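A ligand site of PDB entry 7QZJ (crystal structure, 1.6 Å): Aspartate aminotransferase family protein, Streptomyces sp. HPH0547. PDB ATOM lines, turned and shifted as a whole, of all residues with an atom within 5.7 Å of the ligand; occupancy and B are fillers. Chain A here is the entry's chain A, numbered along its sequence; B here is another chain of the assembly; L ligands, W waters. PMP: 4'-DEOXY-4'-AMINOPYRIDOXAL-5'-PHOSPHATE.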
ATOM      1  N   MET A  79     -25.568 -12.136  27.061  1.00  0.00           N
ATOM      2  CA  MET A  79     -24.130 -12.361  26.812  1.00  0.00           C
ATOM      3  C   MET A  79     -23.397 -11.076  26.432  1.00  0.00           C
ATOM      4  O   MET A  79     -22.386 -11.122  25.729  1.00  0.00           O
ATOM      5  CB  MET A  79     -23.910 -13.415  25.726  1.00  0.00           C
ATOM      6  CG  MET A  79     -24.722 -14.686  25.912  1.00  0.00           C
ATOM      7  SD  MET A  79     -24.296 -16.008  24.751  1.00  0.00           S
ATOM      8  CE  MET A  79     -24.614 -15.245  23.159  1.00  0.00           C
ATOM      9  N   ASN A 136     -26.348  -1.932  13.691  1.00  0.00           N
ATOM     10  CA  ASN A 136     -27.099  -2.154  14.926  1.00  0.00           C
ATOM     11  C   ASN A 136     -26.792  -3.467  15.593  1.00  0.00           C
ATOM     12  O   ASN A 136     -26.839  -3.545  16.805  1.00  0.00           O
ATOM     13  CB  ASN A 136     -28.602  -2.090  14.675  1.00  0.00           C
ATOM     14  CG  ASN A 136     -29.039  -0.797  14.014  1.00  0.00           C
ATOM     15  OD1 ASN A 136     -28.954   0.271  14.608  1.00  0.00           O
ATOM     16  ND2 ASN A 136     -29.482  -0.886  12.774  1.00  0.00           N
ATOM     17  N   SER A 137     -26.524  -4.525  14.831  1.00  0.00           N
ATOM     18  CA  SER A 137     -26.404  -5.879  15.360  1.00  0.00           C
ATOM     19  C   SER A 137     -25.187  -6.586  14.795  1.00  0.00           C
ATOM     20  O   SER A 137     -24.617  -6.200  13.769  1.00  0.00           O
ATOM     21  CB  SER A 137     -27.626  -6.712  15.004  1.00  0.00           C
ATOM     22  OG  SER A 137     -27.721  -6.905  13.593  1.00  0.00           O
ATOM     23  N   GLY A 138     -24.830  -7.700  15.439  1.00  0.00           N
ATOM     24  CA  GLY A 138     -23.756  -8.534  14.919  1.00  0.00           C
ATOM     25  C   GLY A 138     -24.099  -9.159  13.563  1.00  0.00           C
ATOM     26  O   GLY A 138     -23.230  -9.313  12.712  1.00  0.00           O
ATOM     27  N   SER A 139     -25.383  -9.437  13.339  1.00  0.00           N
ATOM     28  CA  SER A 139     -25.840  -9.985  12.051  1.00  0.00           C
ATOM     29  C   SER A 139     -25.656  -8.966  10.943  1.00  0.00           C
ATOM     30  O   SER A 139     -25.195  -9.316   9.835  1.00  0.00           O
ATOM     31  CB  SER A 139     -27.309 -10.418  12.084  1.00  0.00           C
ATOM     32  OG  SER A 139     -27.551 -11.452  13.030  1.00  0.00           O
ATOM     33  N   GLU A 140     -26.010  -7.707  11.213  1.00  0.00           N
ATOM     34  CA  GLU A 140     -25.779  -6.649  10.222  1.00  0.00           C
ATOM     35  C   GLU A 140     -24.265  -6.448   9.969  1.00  0.00           C
ATOM     36  O   GLU A 140     -23.829  -6.170   8.859  1.00  0.00           O
ATOM     37  CB  GLU A 140     -26.428  -5.333  10.659  1.00  0.00           C
ATOM     38  CG  GLU A 140     -27.960  -5.349  10.687  1.00  0.00           C
ATOM     39  CD  GLU A 140     -28.526  -4.122  11.389  1.00  0.00           C
ATOM     40  OE1 GLU A 140     -27.769  -3.452  12.106  1.00  0.00           O
ATOM     41  OE2 GLU A 140     -29.742  -3.838  11.225  1.00  0.00           O
ATOM     42  N   THR A 142     -22.022  -8.789  10.091  1.00  0.00           N
ATOM     43  CA  THR A 142     -21.721  -9.886   9.159  1.00  0.00           C
ATOM     44  C   THR A 142     -22.176  -9.558   7.724  1.00  0.00           C
ATOM     45  O   THR A 142     -21.415  -9.724   6.755  1.00  0.00           O
ATOM     46  CB  THR A 142     -22.313 -11.195   9.645  1.00  0.00           C
ATOM     47  OG1 THR A 142     -21.685 -11.546  10.882  1.00  0.00           O
ATOM     48  CG2 THR A 142     -22.130 -12.319   8.642  1.00  0.00           C
ATOM     49  N   TYR A 170     -20.977 -19.391  14.188  1.00  0.00           N
ATOM     50  CA  TYR A 170     -22.260 -18.659  14.154  1.00  0.00           C
ATOM     51  C   TYR A 170     -21.939 -17.200  13.979  1.00  0.00           C
ATOM     52  O   TYR A 170     -21.116 -16.643  14.702  1.00  0.00           O
ATOM     53  CB  TYR A 170     -23.082 -18.871  15.414  1.00  0.00           C
ATOM     54  CG  TYR A 170     -24.386 -18.114  15.398  1.00  0.00           C
ATOM     55  CD1 TYR A 170     -25.482 -18.638  14.719  1.00  0.00           C
ATOM     56  CD2 TYR A 170     -24.541 -16.891  16.054  1.00  0.00           C
ATOM     57  CE1 TYR A 170     -26.691 -17.968  14.665  1.00  0.00           C
ATOM     58  CE2 TYR A 170     -25.751 -16.209  15.994  1.00  0.00           C
ATOM     59  CZ  TYR A 170     -26.826 -16.741  15.312  1.00  0.00           C
ATOM     60  OH  TYR A 170     -28.036 -16.052  15.264  1.00  0.00           O
ATOM     61  N   HIS A 171     -22.595 -16.584  12.992  1.00  0.00           N
ATOM     62  CA  HIS A 171     -22.297 -15.215  12.600  1.00  0.00           C
ATOM     63  C   HIS A 171     -23.547 -14.343  12.526  1.00  0.00           C
ATOM     64  O   HIS A 171     -23.476 -13.214  12.051  1.00  0.00           O
ATOM     65  CB  HIS A 171     -21.572 -15.235  11.258  1.00  0.00           C
ATOM     66  CG  HIS A 171     -20.288 -16.001  11.333  1.00  0.00           C
ATOM     67  ND1 HIS A 171     -19.237 -15.589  12.125  1.00  0.00           N
ATOM     68  CD2 HIS A 171     -19.925 -17.192  10.812  1.00  0.00           C
ATOM     69  CE1 HIS A 171     -18.264 -16.483  12.048  1.00  0.00           C
ATOM     70  NE2 HIS A 171     -18.653 -17.454  11.255  1.00  0.00           N
ATOM     71  N   GLY A 172     -24.656 -14.851  13.036  1.00  0.00           N
ATOM     72  CA  GLY A 172     -25.929 -14.115  12.993  1.00  0.00           C
ATOM     73  C   GLY A 172     -27.053 -14.846  12.333  1.00  0.00           C
ATOM     74  O   GLY A 172     -26.953 -16.027  11.932  1.00  0.00           O
ATOM     75  N   THR A 173     -28.174 -14.129  12.209  1.00  0.00           N
ATOM     76  CA  THR A 173     -29.469 -14.735  11.956  1.00  0.00           C
ATOM     77  C   THR A 173     -30.106 -14.391  10.602  1.00  0.00           C
ATOM     78  O   THR A 173     -31.134 -14.942  10.259  1.00  0.00           O
ATOM     79  CB  THR A 173     -30.432 -14.387  13.110  1.00  0.00           C
ATOM     80  OG1 THR A 173     -31.641 -15.128  12.971  1.00  0.00           O
ATOM     81  CG2 THR A 173     -30.766 -12.903  13.136  1.00  0.00           C
ATOM     82  N   GLU A 237     -14.571 -16.985  14.147  1.00  0.00           N
ATOM     83  CA  GLU A 237     -14.510 -16.533  15.534  1.00  0.00           C
ATOM     84  C   GLU A 237     -13.196 -17.032  16.133  1.00  0.00           C
ATOM     85  O   GLU A 237     -12.721 -18.106  15.731  1.00  0.00           O
ATOM     86  CB  GLU A 237     -15.635 -17.151  16.356  1.00  0.00           C
ATOM     87  CG  GLU A 237     -17.063 -16.799  15.900  1.00  0.00           C
ATOM     88  CD  GLU A 237     -18.083 -17.813  16.398  1.00  0.00           C
ATOM     89  OE1 GLU A 237     -18.383 -18.759  15.643  1.00  0.00           O
ATOM     90  OE2 GLU A 237     -18.580 -17.717  17.542  1.00  0.00           O
ATOM     91  N   ASN A 241     -18.568 -19.447  20.019  1.00  0.00           N
ATOM     92  CA  ASN A 241     -19.574 -19.201  21.057  1.00  0.00           C
ATOM     93  C   ASN A 241     -20.760 -20.160  20.913  1.00  0.00           C
ATOM     94  O   ASN A 241     -20.850 -21.185  21.620  1.00  0.00           O
ATOM     95  CB  ASN A 241     -19.986 -17.724  20.987  1.00  0.00           C
ATOM     96  CG  ASN A 241     -21.195 -17.389  21.834  1.00  0.00           C
ATOM     97  OD1 ASN A 241     -21.413 -17.970  22.880  1.00  0.00           O
ATOM     98  ND2 ASN A 241     -21.987 -16.403  21.384  1.00  0.00           N
ATOM     99  N   VAL A 242     -21.667 -19.896  19.965  1.00  0.00           N
ATOM    100  CA  VAL A 242     -22.871 -20.730  19.787  1.00  0.00           C
ATOM    101  C   VAL A 242     -22.525 -22.190  19.454  1.00  0.00           C
ATOM    102  O   VAL A 242     -23.239 -23.107  19.833  1.00  0.00           O
ATOM    103  CB  VAL A 242     -23.816 -20.119  18.728  1.00  0.00           C
ATOM    104  CG1 VAL A 242     -24.961 -21.071  18.366  1.00  0.00           C
ATOM    105  CG2 VAL A 242     -24.336 -18.792  19.251  1.00  0.00           C
ATOM    106  N   ASP A 270     -14.496 -12.512  13.585  1.00  0.00           N
ATOM    107  CA  ASP A 270     -15.772 -12.188  14.219  1.00  0.00           C
ATOM    108  C   ASP A 270     -15.512 -12.100  15.733  1.00  0.00           C
ATOM    109  O   ASP A 270     -15.431 -13.118  16.420  1.00  0.00           O
ATOM    110  CB  ASP A 270     -16.822 -13.235  13.848  1.00  0.00           C
ATOM    111  CG  ASP A 270     -18.207 -12.934  14.434  1.00  0.00           C
ATOM    112  OD1 ASP A 270     -18.288 -12.197  15.451  1.00  0.00           O
ATOM    113  OD2 ASP A 270     -19.204 -13.450  13.883  1.00  0.00           O
ATOM    114  N   GLU A 271     -15.446 -10.855  16.226  1.00  0.00           N
ATOM    115  CA  GLU A 271     -15.298 -10.540  17.664  1.00  0.00           C
ATOM    116  C   GLU A 271     -16.630 -10.105  18.303  1.00  0.00           C
ATOM    117  O   GLU A 271     -16.635  -9.493  19.364  1.00  0.00           O
ATOM    118  CB  GLU A 271     -14.260  -9.440  17.864  1.00  0.00           C
ATOM    119  CG  GLU A 271     -12.840  -9.876  17.549  1.00  0.00           C
ATOM    120  CD  GLU A 271     -12.211 -10.736  18.638  1.00  0.00           C
ATOM    121  OE1 GLU A 271     -12.655 -10.710  19.812  1.00  0.00           O
ATOM    122  OE2 GLU A 271     -11.217 -11.453  18.333  1.00  0.00           O
ATOM    123  N   VAL A 272     -17.747 -10.443  17.661  1.00  0.00           N
ATOM    124  CA  VAL A 272     -19.076 -10.063  18.209  1.00  0.00           C
ATOM    125  C   VAL A 272     -19.254 -10.543  19.674  1.00  0.00           C
ATOM    126  O   VAL A 272     -19.696  -9.768  20.537  1.00  0.00           O
ATOM    127  CB  VAL A 272     -20.213 -10.512  17.281  1.00  0.00           C
ATOM    128  CG1 VAL A 272     -21.564 -10.494  18.009  1.00  0.00           C
ATOM    129  CG2 VAL A 272     -20.249  -9.648  16.022  1.00  0.00           C
ATOM    130  N   PHE A 273     -18.846 -11.788  19.973  1.00  0.00           N
ATOM    131  CA  PHE A 273     -18.940 -12.331  21.323  1.00  0.00           C
ATOM    132  C   PHE A 273     -17.662 -12.029  22.141  1.00  0.00           C
ATOM    133  O   PHE A 273     -17.755 -11.648  23.288  1.00  0.00           O
ATOM    134  CB  PHE A 273     -19.215 -13.833  21.275  1.00  0.00           C
ATOM    135  CG  PHE A 273     -19.212 -14.491  22.641  1.00  0.00           C
ATOM    136  CD1 PHE A 273     -20.265 -14.276  23.533  1.00  0.00           C
ATOM    137  CD2 PHE A 273     -18.141 -15.263  23.062  1.00  0.00           C
ATOM    138  CE1 PHE A 273     -20.255 -14.857  24.787  1.00  0.00           C
ATOM    139  CE2 PHE A 273     -18.131 -15.843  24.316  1.00  0.00           C
ATOM    140  CZ  PHE A 273     -19.193 -15.642  25.183  1.00  0.00           C
ATOM    141  N   SER A 298     -19.807  -6.364  18.490  1.00  0.00           N
ATOM    142  CA  SER A 298     -21.145  -5.995  19.003  1.00  0.00           C
ATOM    143  C   SER A 298     -21.140  -6.346  20.496  1.00  0.00           C
ATOM    144  O   SER A 298     -20.102  -6.213  21.138  1.00  0.00           O
ATOM    145  CB  SER A 298     -22.240  -6.692  18.207  1.00  0.00           C
ATOM    146  OG  SER A 298     -23.532  -6.218  18.595  1.00  0.00           O
ATOM    147  N   LYS A 299     -22.261  -6.814  21.040  1.00  0.00           N
ATOM    148  CA  LYS A 299     -22.391  -7.247  22.435  1.00  0.00           C
ATOM    149  C   LYS A 299     -21.814  -6.286  23.496  1.00  0.00           C
ATOM    150  O   LYS A 299     -22.407  -5.221  23.739  1.00  0.00           O
ATOM    151  CB  LYS A 299     -21.920  -8.700  22.606  1.00  0.00           C
ATOM    152  CG  LYS A 299     -22.841  -9.649  21.876  1.00  0.00           C
ATOM    153  CD  LYS A 299     -22.503 -11.089  22.147  1.00  0.00           C
ATOM    154  CE  LYS A 299     -23.650 -12.031  21.956  1.00  0.00           C
ATOM    155  NZ  LYS A 299     -24.322 -11.795  20.672  1.00  0.00           N
ATOM    156  N   ASN B 136     -34.001  -5.074  15.408  1.00  0.00           N
ATOM    157  CA  ASN B 136     -33.366  -3.764  15.602  1.00  0.00           C
ATOM    158  C   ASN B 136     -33.612  -2.748  14.487  1.00  0.00           C
ATOM    159  O   ASN B 136     -33.701  -1.569  14.761  1.00  0.00           O
ATOM    160  CB  ASN B 136     -31.849  -3.875  15.808  1.00  0.00           C
ATOM    161  CG  ASN B 136     -31.454  -4.853  16.893  1.00  0.00           C
ATOM    162  OD1 ASN B 136     -31.661  -4.588  18.087  1.00  0.00           O
ATOM    163  ND2 ASN B 136     -30.916  -5.989  16.502  1.00  0.00           N
ATOM    164  N   GLU B 140     -33.615  -5.859   9.135  1.00  0.00           N
ATOM    165  CA  GLU B 140     -33.842  -7.115   9.886  1.00  0.00           C
ATOM    166  C   GLU B 140     -35.311  -7.539   9.859  1.00  0.00           C
ATOM    167  O   GLU B 140     -35.635  -8.718   9.808  1.00  0.00           O
ATOM    168  CB  GLU B 140     -33.342  -7.002  11.332  1.00  0.00           C
ATOM    169  CG  GLU B 140     -31.820  -6.845  11.485  1.00  0.00           C
ATOM    170  CD  GLU B 140     -31.415  -6.453  12.893  1.00  0.00           C
ATOM    171  OE1 GLU B 140     -32.289  -6.016  13.644  1.00  0.00           O
ATOM    172  OE2 GLU B 140     -30.229  -6.598  13.279  1.00  0.00           O
ATOM    173  N   GLY B 333     -33.617 -14.752  15.220  1.00  0.00           N
ATOM    174  CA  GLY B 333     -33.557 -13.890  16.400  1.00  0.00           C
ATOM    175  C   GLY B 333     -32.215 -13.210  16.560  1.00  0.00           C
ATOM    176  O   GLY B 333     -31.158 -13.787  16.288  1.00  0.00           O
ATOM    177  N   HIS B 334     -32.279 -11.984  17.091  1.00  0.00           N
ATOM    178  CA  HIS B 334     -31.137 -11.145  17.376  1.00  0.00           C
ATOM    179  C   HIS B 334     -30.948 -11.018  18.881  1.00  0.00           C
ATOM    180  O   HIS B 334     -31.920 -10.978  19.644  1.00  0.00           O
ATOM    181  CB  HIS B 334     -31.330  -9.732  16.813  1.00  0.00           C
ATOM    182  CG  HIS B 334     -31.398  -9.688  15.318  1.00  0.00           C
ATOM    183  ND1 HIS B 334     -30.279  -9.676  14.518  1.00  0.00           N
ATOM    184  CD2 HIS B 334     -32.472  -9.678  14.481  1.00  0.00           C
ATOM    185  CE1 HIS B 334     -30.668  -9.668  13.245  1.00  0.00           C
ATOM    186  NE2 HIS B 334     -31.979  -9.669  13.202  1.00  0.00           N
ATOM    187  N   THR B 335     -29.688 -10.876  19.272  1.00  0.00           N
ATOM    188  CA  THR B 335     -29.296 -10.619  20.669  1.00  0.00           C
ATOM    189  C   THR B 335     -30.095  -9.532  21.371  1.00  0.00           C
ATOM    190  O   THR B 335     -30.584  -9.756  22.499  1.00  0.00           O
ATOM    191  CB  THR B 335     -27.793 -10.274  20.724  1.00  0.00           C
ATOM    192  OG1 THR B 335     -27.063 -11.412  20.237  1.00  0.00           O
ATOM    193  CG2 THR B 335     -27.296  -9.919  22.130  1.00  0.00           C
ATOM    194  N   THR B 336     -30.243  -8.381  20.716  1.00  0.00           N
ATOM    195  CA  THR B 336     -30.963  -7.253  21.304  1.00  0.00           C
ATOM    196  C   THR B 336     -32.368  -7.090  20.716  1.00  0.00           C
ATOM    197  O   THR B 336     -32.990  -6.052  20.940  1.00  0.00           O
ATOM    198  CB  THR B 336     -30.195  -5.938  21.238  1.00  0.00           C
ATOM    199  OG1 THR B 336     -29.941  -5.582  19.880  1.00  0.00           O
ATOM    200  CG2 THR B 336     -28.854  -6.027  21.943  1.00  0.00           C
HETATM  201  N1  PMP L   1     -21.446 -13.247  15.660  1.00  0.00           N
HETATM  202  C2  PMP L   1     -21.208 -13.944  16.792  1.00  0.00           C
HETATM  203  C2A PMP L   1     -19.847 -14.509  17.077  1.00  0.00           C
HETATM  204  C3  PMP L   1     -22.301 -14.097  17.780  1.00  0.00           C
HETATM  205  O3  PMP L   1     -22.102 -14.821  18.924  1.00  0.00           O
HETATM  206  C4  PMP L   1     -23.624 -13.484  17.447  1.00  0.00           C
HETATM  207  C4A PMP L   1     -24.838 -13.608  18.318  1.00  0.00           C
HETATM  208  N4A PMP L   1     -24.758 -14.674  19.294  1.00  0.00           N
HETATM  209  C5  PMP L   1     -23.752 -12.761  16.154  1.00  0.00           C
HETATM  210  C6  PMP L   1     -22.626 -12.683  15.311  1.00  0.00           C
HETATM  211  C5A PMP L   1     -25.076 -12.118  15.726  1.00  0.00           C
HETATM  212  O4P PMP L   1     -25.340 -10.934  16.486  1.00  0.00           O
HETATM  213  P   PMP L   1     -26.855 -10.394  16.656  1.00  0.00           P
HETATM  214  O1P PMP L   1     -26.524  -9.098  17.373  1.00  0.00           O
HETATM  215  O2P PMP L   1     -27.441 -10.222  15.258  1.00  0.00           O
HETATM  216  O3P PMP L   1     -27.556 -11.422  17.461  1.00  0.00           O
HETATM  217  O   HOH W   1     -28.799  -7.778  18.190  1.00  0.00           O
HETATM  218  O   HOH W   2     -28.497 -13.778  16.596  1.00  0.00           O
HETATM  219  O   HOH W   3     -21.337 -17.594  18.104  1.00  0.00           O
HETATM  220  O   HOH W   4     -25.018  -8.283  19.512  1.00  0.00           O
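Merely in contact with the ligand: His 171 (3.4 Å), Val 272 (3.4 Å), Tyr 170 (3.4 Å), Glu 237 (3.5 Å), Gly 172 (3.5 Å), Ser 137 (3.5 Å), Phe 273 (3.9 Å) and Met 79 (3.9 Å). Hydrophobic or aromatic side chains that line the ligand: Met 79, Tyr 170, Val 272, Phe 273 and His 334 of chain B. 15 residues have an atom within 4 Å of the ligand: Met 79, Ser 137, Gly 138, Ser 139, Tyr 170, His 171, Gly 172, Glu 237, Asn 241, Asp 270, Val 272, Phe 273, Lys 299, His 334 of chain B and Thr 335 of chain B.
O2P of the ligand sits at hydrogen-bond distance from N of Ser 139, 2.9 Å away. OG of Ser 139 sits at hydrogen-bond distance from O2P of the ligand, at 2.5 Å. O3P of the ligand is in hydrogen-bond range of N of Thr 335 of chain B (2.9 Å). The side-chain hydroxyl (OG1) of Thr 335 of chain B lies within hydrogen-bond range of an oxygen (O3P) of the ligand (2.8 Å). The side-chain carboxylate of Asp 270 lies within hydrogen-bond range of a nitrogen (N1) of the ligand, at 2.9 Å. The backbone NH (N) of Gly 138 lies within hydrogen-bond range of an oxygen (O1P) of the ligand (2.9 Å). An oxygen (O3) of the ligand sits at hydrogen-bond distance from the side-chain amide nitrogen of Asn 241, 2.9 Å away. A ring nitrogen (ND1) of His 334 of chain B is in hydrogen-bond range of an oxygen (O2P) of the ligand, at 3.0 Å. The side-chain amino group (NZ) of Lys 299 lies close to a nitrogen (N4A) of the ligand.
The backbone NH of Thr 173 is in hydrogen-bond range of the side-chain hydroxyl of Ser 139. The side-chain carboxylate of Asp 270 is in hydrogen-bond range of a ring nitrogen (ND1) of His 171, 2.8 Å away. The backbone carbonyl oxygen (O) of Gly 138 lies within hydrogen-bond range of the side-chain hydroxyl (OG1) of Thr 142, at 3.3 Å. ND1 of His 334 of chain B sits close to OE2 of Glu 140 of chain B. The side-chain hydroxyl (OG1) of Thr 142 is in hydrogen-bond range of the backbone carbonyl oxygen (O) of His 171 (2.7 Å). The backbone NH of Tyr 170 lies within hydrogen-bond range of the side-chain carboxylate of Glu 237 (3.0 Å). The side-chain hydroxyl (OG) of Ser 137 sits at hydrogen-bond distance from the backbone NH (N) of Glu 140 of chain A, at 3.0 Å. The side-chain hydroxyl (OG) of Ser 137 is in hydrogen-bond range of the side-chain carboxylate (OE2) of Glu 140 of chain B, at 2.5 Å.
Water W2 lies within hydrogen-bond range of OH of Tyr 170 (2.7 Å), O of Gly 333 of chain B (2.7 Å) and O3P of the ligand (2.7 Å). Water W4 lies within hydrogen-bond range of OG of Ser 298 (2.7 Å), O1P of the ligand (2.7 Å) and N of Lys 299 (3.5 Å). Water W3 lies within hydrogen-bond range of the side-chain carboxylate (OE2) of Glu 237 (2.8 Å), the backbone NH (N) of Val 242 (3.0 Å) and an oxygen (O3) of the ligand (3.0 Å).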
